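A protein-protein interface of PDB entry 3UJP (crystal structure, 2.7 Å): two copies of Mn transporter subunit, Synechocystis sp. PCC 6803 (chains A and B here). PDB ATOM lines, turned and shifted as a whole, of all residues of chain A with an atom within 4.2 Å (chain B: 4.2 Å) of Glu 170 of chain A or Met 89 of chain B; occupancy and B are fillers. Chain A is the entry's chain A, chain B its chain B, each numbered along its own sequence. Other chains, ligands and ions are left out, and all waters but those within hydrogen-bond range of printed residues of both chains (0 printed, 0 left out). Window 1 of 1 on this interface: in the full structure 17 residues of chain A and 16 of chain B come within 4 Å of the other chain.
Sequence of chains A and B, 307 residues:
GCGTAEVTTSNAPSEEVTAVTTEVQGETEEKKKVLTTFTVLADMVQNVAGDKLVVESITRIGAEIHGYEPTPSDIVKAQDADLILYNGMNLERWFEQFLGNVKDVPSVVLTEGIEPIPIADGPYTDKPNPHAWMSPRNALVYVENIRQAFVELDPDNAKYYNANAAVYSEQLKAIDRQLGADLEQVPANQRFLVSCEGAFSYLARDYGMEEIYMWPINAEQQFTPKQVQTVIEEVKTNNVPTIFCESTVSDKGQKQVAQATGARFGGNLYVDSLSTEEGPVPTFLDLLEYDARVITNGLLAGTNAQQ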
ATOM      1  N   ALA A 166      13.670  18.625 -13.224  1.00  0.00           N
ATOM      2  CA  ALA A 166      12.625  19.422 -13.865  1.00  0.00           C
ATOM      3  C   ALA A 166      11.321  18.630 -13.993  1.00  0.00           C
ATOM      4  O   ALA A 166      10.276  19.020 -13.457  1.00  0.00           O
ATOM      5  CB  ALA A 166      13.103  19.872 -15.243  1.00  0.00           C
ATOM      6  N   VAL A 167      11.400  17.520 -14.724  1.00  0.00           N
ATOM      7  CA  VAL A 167      10.270  16.631 -14.936  1.00  0.00           C
ATOM      8  C   VAL A 167       9.708  16.067 -13.621  1.00  0.00           C
ATOM      9  O   VAL A 167       8.511  15.955 -13.458  1.00  0.00           O
ATOM     10  CB  VAL A 167      10.652  15.476 -15.886  1.00  0.00           C
ATOM     11  CG1 VAL A 167       9.622  14.349 -15.852  1.00  0.00           C
ATOM     12  CG2 VAL A 167      10.848  15.997 -17.280  1.00  0.00           C
ATOM     13  N   TYR A 168      10.554  15.706 -12.667  1.00  0.00           N
ATOM     14  CA  TYR A 168      10.033  15.183 -11.403  1.00  0.00           C
ATOM     15  C   TYR A 168       9.406  16.341 -10.617  1.00  0.00           C
ATOM     16  O   TYR A 168       8.319  16.196 -10.069  1.00  0.00           O
ATOM     17  CB  TYR A 168      11.127  14.447 -10.604  1.00  0.00           C
ATOM     18  CG  TYR A 168      10.592  13.450  -9.608  1.00  0.00           C
ATOM     19  CD1 TYR A 168       9.671  12.501  -9.993  1.00  0.00           C
ATOM     20  CD2 TYR A 168      11.013  13.446  -8.271  1.00  0.00           C
ATOM     21  CE1 TYR A 168       9.165  11.558  -9.073  1.00  0.00           C
ATOM     22  CE2 TYR A 168      10.506  12.519  -7.342  1.00  0.00           C
ATOM     23  CZ  TYR A 168       9.584  11.566  -7.750  1.00  0.00           C
ATOM     24  OH  TYR A 168       9.054  10.635  -6.862  1.00  0.00           O
ATOM     25  N   SER A 169      10.075  17.491 -10.575  1.00  0.00           N
ATOM     26  CA  SER A 169       9.533  18.653  -9.872  1.00  0.00           C
ATOM     27  C   SER A 169       8.134  18.955 -10.389  1.00  0.00           C
ATOM     28  O   SER A 169       7.211  19.246  -9.634  1.00  0.00           O
ATOM     29  CB  SER A 169      10.417  19.890 -10.067  1.00  0.00           C
ATOM     30  OG  SER A 169      11.648  19.786  -9.374  1.00  0.00           O
ATOM     31  N   GLU A 170       7.997  18.877 -11.705  1.00  0.00           N
ATOM     32  CA  GLU A 170       6.750  19.190 -12.364  1.00  0.00           C
ATOM     33  C   GLU A 170       5.639  18.205 -12.044  1.00  0.00           C
ATOM     34  O   GLU A 170       4.489  18.587 -11.942  1.00  0.00           O
ATOM     35  CB  GLU A 170       6.960  19.214 -13.867  1.00  0.00           C
ATOM     36  CG  GLU A 170       5.723  18.773 -14.604  1.00  0.00           C
ATOM     37  CD  GLU A 170       5.974  18.511 -16.068  1.00  0.00           C
ATOM     38  OE1 GLU A 170       6.481  17.410 -16.403  1.00  0.00           O
ATOM     39  OE2 GLU A 170       5.648  19.408 -16.877  1.00  0.00           O
ATOM     40  N   GLN A 171       5.974  16.933 -11.915  1.00  0.00           N
ATOM     41  CA  GLN A 171       4.966  15.914 -11.622  1.00  0.00           C
ATOM     42  C   GLN A 171       4.607  15.924 -10.149  1.00  0.00           C
ATOM     43  O   GLN A 171       3.559  15.423  -9.767  1.00  0.00           O
ATOM     44  CB  GLN A 171       5.465  14.521 -11.987  1.00  0.00           C
ATOM     45  CG  GLN A 171       5.782  14.329 -13.442  1.00  0.00           C
ATOM     46  CD  GLN A 171       6.693  13.161 -13.646  1.00  0.00           C
ATOM     47  OE1 GLN A 171       7.077  12.514 -12.684  1.00  0.00           O
ATOM     48  NE2 GLN A 171       7.055  12.883 -14.901  1.00  0.00           N
ATOM     49  N   LEU A 172       5.508  16.464  -9.332  1.00  0.00           N
ATOM     50  CA  LEU A 172       5.229  16.738  -7.923  1.00  0.00           C
ATOM     51  C   LEU A 172       4.157  17.828  -7.766  1.00  0.00           C
ATOM     52  O   LEU A 172       3.259  17.697  -6.919  1.00  0.00           O
ATOM     53  CB  LEU A 172       6.497  17.203  -7.208  1.00  0.00           C
ATOM     54  CG  LEU A 172       7.248  16.344  -6.195  1.00  0.00           C
ATOM     55  CD1 LEU A 172       6.465  15.134  -5.739  1.00  0.00           C
ATOM     56  CD2 LEU A 172       8.561  15.934  -6.789  1.00  0.00           C
ATOM     57  N   LYS A 173       4.270  18.906  -8.558  1.00  0.00           N
ATOM     58  CA  LYS A 173       3.290  20.011  -8.515  1.00  0.00           C
ATOM     59  C   LYS A 173       1.888  19.593  -8.982  1.00  0.00           C
ATOM     60  O   LYS A 173       0.885  19.958  -8.366  1.00  0.00           O
ATOM     61  CB  LYS A 173       3.812  21.251  -9.241  1.00  0.00           C
ATOM     62  CG  LYS A 173       5.152  21.757  -8.663  1.00  0.00           C
ATOM     63  CD  LYS A 173       6.133  22.194  -9.761  1.00  0.00           C
ATOM     64  CE  LYS A 173       6.938  23.415  -9.341  1.00  0.00           C
ATOM     65  NZ  LYS A 173       7.962  23.814 -10.366  1.00  0.00           N
ATOM     66  N   ALA A 174       1.833  18.775 -10.021  1.00  0.00           N
ATOM     67  CA  ALA A 174       0.572  18.189 -10.442  1.00  0.00           C
ATOM     68  C   ALA A 174      -0.161  17.506  -9.296  1.00  0.00           C
ATOM     69  O   ALA A 174      -1.282  17.877  -8.978  1.00  0.00           O
ATOM     70  CB  ALA A 174       0.773  17.225 -11.597  1.00  0.00           C
ATOM     71  N   GLY B  88       2.932  17.058 -20.098  1.00  0.00           N
ATOM     72  CA  GLY B  88       3.947  17.426 -19.128  1.00  0.00           C
ATOM     73  C   GLY B  88       5.220  17.836 -19.849  1.00  0.00           C
ATOM     74  O   GLY B  88       5.205  18.039 -21.059  1.00  0.00           O
ATOM     75  N   MET B  89       6.324  17.932 -19.108  1.00  0.00           N
ATOM     76  CA  MET B  89       7.619  18.306 -19.664  1.00  0.00           C
ATOM     77  C   MET B  89       7.505  19.633 -20.396  1.00  0.00           C
ATOM     78  O   MET B  89       8.203  19.901 -21.371  1.00  0.00           O
ATOM     79  CB  MET B  89       8.168  17.197 -20.560  1.00  0.00           C
ATOM     80  CG  MET B  89       8.225  15.842 -19.842  1.00  0.00           C
ATOM     81  SD  MET B  89       8.786  14.414 -20.808  1.00  0.00           S
ATOM     82  CE  MET B  89      10.381  14.993 -21.314  1.00  0.00           C
ATOM     83  N   ASN B  90       6.614  20.463 -19.885  1.00  0.00           N
ATOM     84  CA  ASN B  90       6.457  21.803 -20.381  1.00  0.00           C
ATOM     85  C   ASN B  90       6.141  21.796 -21.867  1.00  0.00           C
ATOM     86  O   ASN B  90       6.328  22.815 -22.540  1.00  0.00           O
ATOM     87  CB  ASN B  90       7.744  22.565 -20.153  1.00  0.00           C
ATOM     88  CG  ASN B  90       7.518  24.034 -20.071  1.00  0.00           C
ATOM     89  OD1 ASN B  90       6.444  24.478 -19.661  1.00  0.00           O
ATOM     90  ND2 ASN B  90       8.528  24.814 -20.462  1.00  0.00           N
ATOM     91  N   LEU B  91       5.696  20.650 -22.393  1.00  0.00           N
ATOM     92  CA  LEU B  91       5.364  20.578 -23.813  1.00  0.00           C
ATOM     93  C   LEU B  91       4.381  21.677 -24.058  1.00  0.00           C
ATOM     94  O   LEU B  91       4.668  22.636 -24.792  1.00  0.00           O
ATOM     95  CB  LEU B  91       4.701  19.266 -24.211  1.00  0.00           C
ATOM     96  CG  LEU B  91       4.061  19.397 -25.594  1.00  0.00           C
ATOM     97  CD1 LEU B  91       5.168  19.451 -26.582  1.00  0.00           C
ATOM     98  CD2 LEU B  91       3.107  18.279 -25.940  1.00  0.00           C
ATOM     99  N   THR B 111       3.162  11.661 -18.938  1.00  0.00           N
ATOM    100  CA  THR B 111       4.586  11.554 -19.058  1.00  0.00           C
ATOM    101  C   THR B 111       5.274  10.971 -17.810  1.00  0.00           C
ATOM    102  O   THR B 111       6.465  10.695 -17.849  1.00  0.00           O
ATOM    103  CB  THR B 111       5.163  12.924 -19.347  1.00  0.00           C
ATOM    104  OG1 THR B 111       5.844  12.873 -20.601  1.00  0.00           O
ATOM    105  CG2 THR B 111       6.112  13.386 -18.239  1.00  0.00           C
ATOM    106  N   PRO B 116      13.514  11.870 -19.636  1.00  0.00           N
ATOM    107  CA  PRO B 116      13.792  12.709 -20.805  1.00  0.00           C
ATOM    108  C   PRO B 116      15.221  12.646 -21.409  1.00  0.00           C
ATOM    109  O   PRO B 116      16.197  12.333 -20.720  1.00  0.00           O
ATOM    110  CB  PRO B 116      13.507  14.134 -20.298  1.00  0.00           C
ATOM    111  CG  PRO B 116      13.535  14.042 -18.780  1.00  0.00           C
ATOM    112  CD  PRO B 116      13.235  12.639 -18.413  1.00  0.00           C
ATOM    113  N   PRO B 128      13.794  19.493 -20.623  1.00  0.00           N
ATOM    114  CA  PRO B 128      13.495  18.179 -21.205  1.00  0.00           C
ATOM    115  C   PRO B 128      12.797  18.267 -22.558  1.00  0.00           C
ATOM    116  O   PRO B 128      11.890  19.097 -22.682  1.00  0.00           O
ATOM    117  CB  PRO B 128      12.537  17.559 -20.186  1.00  0.00           C
ATOM    118  CG  PRO B 128      12.444  18.528 -19.027  1.00  0.00           C
ATOM    119  CD  PRO B 128      12.856  19.859 -19.553  1.00  0.00           C
ATOM    120  N   ASN B 129      13.190  17.428 -23.524  1.00  0.00           N
ATOM    121  CA  ASN B 129      12.529  17.313 -24.827  1.00  0.00           C
ATOM    122  C   ASN B 129      11.172  16.635 -24.650  1.00  0.00           C
ATOM    123  O   ASN B 129      11.103  15.427 -24.444  1.00  0.00           O
ATOM    124  CB  ASN B 129      13.393  16.489 -25.787  1.00  0.00           C
ATOM    125  CG  ASN B 129      12.861  16.477 -27.221  1.00  0.00           C
ATOM    126  OD1 ASN B 129      11.753  16.917 -27.490  1.00  0.00           O
ATOM    127  ND2 ASN B 129      13.661  15.964 -28.141  1.00  0.00           N
ATOM    128  N   PRO B 130      10.072  17.410 -24.750  1.00  0.00           N
ATOM    129  CA  PRO B 130       8.748  16.877 -24.364  1.00  0.00           C
ATOM    130  C   PRO B 130       8.157  15.826 -25.309  1.00  0.00           C
ATOM    131  O   PRO B 130       7.241  15.118 -24.920  1.00  0.00           O
ATOM    132  CB  PRO B 130       7.846  18.118 -24.343  1.00  0.00           C
ATOM    133  CG  PRO B 130       8.534  19.111 -25.266  1.00  0.00           C
ATOM    134  CD  PRO B 130      10.007  18.794 -25.269  1.00  0.00           C
ATOM    135  N   TYR B 202      13.525  11.091 -29.512  1.00  0.00           N
ATOM    136  CA  TYR B 202      13.234   9.795 -28.923  1.00  0.00           C
ATOM    137  C   TYR B 202      13.145   8.719 -29.989  1.00  0.00           C
ATOM    138  O   TYR B 202      13.351   7.550 -29.709  1.00  0.00           O
ATOM    139  CB  TYR B 202      11.963   9.845 -28.078  1.00  0.00           C
ATOM    140  CG  TYR B 202      12.031  10.819 -26.923  1.00  0.00           C
ATOM    141  CD1 TYR B 202      12.387  10.389 -25.660  1.00  0.00           C
ATOM    142  CD2 TYR B 202      11.736  12.168 -27.098  1.00  0.00           C
ATOM    143  CE1 TYR B 202      12.448  11.267 -24.585  1.00  0.00           C
ATOM    144  CE2 TYR B 202      11.786  13.065 -26.038  1.00  0.00           C
ATOM    145  CZ  TYR B 202      12.146  12.606 -24.768  1.00  0.00           C
ATOM    146  OH  TYR B 202      12.230  13.467 -23.677  1.00  0.00           O
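No position is printed for both chains.
Of the 7 pairs that touch across the chains among the printed residues, none has its exchanged pair printed and touching as well.
The side-chain sulfur (SD) of Met 89 of chain B sits at hydrogen-bond distance from the side-chain hydroxyl (OG1) of Thr 111 of chain B, at 3.3 Å.
OE2 of Glu 170 of chain A sits at hydrogen-bond distance from N of Met 89 of chain B, 2.8 Å away.
OE2 of Glu 170 of chain A lies within hydrogen-bond range of N of Asn 90 of chain B, 3.3 Å away.
CG2 of Val 167 of chain A touches CG of Met 89 of chain B, at 3.7 Å.
Pro 116 of chain B touches Val 167 of chain A.
Pro 128 of chain B touches Val 167 of chain A (CG to CG2, 3.5 Å).
Glu 170 of chain A touches Gly 88 of chain B.
CG2 of Thr 111 of chain B touches NE2 of Gln 171 of chain A, 3.5 Å away.
Of the 9 printed residues of chain A, 3 touch a printed residue of chain B.
Hydrophobic or aromatic side chains of chain A that line the printed part of chain B: Val 167.
Of the 10 printed residues of chain B, 6 touch a printed residue of chain A.
Hydrophobic or aromatic side chains of chain B that line the printed part of chain A: Met 89, Pro 116 and Pro 128.
Among the printed residues, no Asp or Glu carboxylate lies within 4 Å of a Lys or Arg side-chain nitrogen of the other chain.
Glu 170 of chain A touches three residues of chain B.
Met 89 of chain B touches just these residues of chain A: Val 167 and Glu 170.
Of the printed residues of chain A, Asn 90 of chain B touches Glu 170 (3.3 Å).
Of the printed residues of chain A, Pro 116 of chain B touches Val 167.
Of the printed residues of chain A, Gly 88 of chain B touches Glu 170 (3.4 Å).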
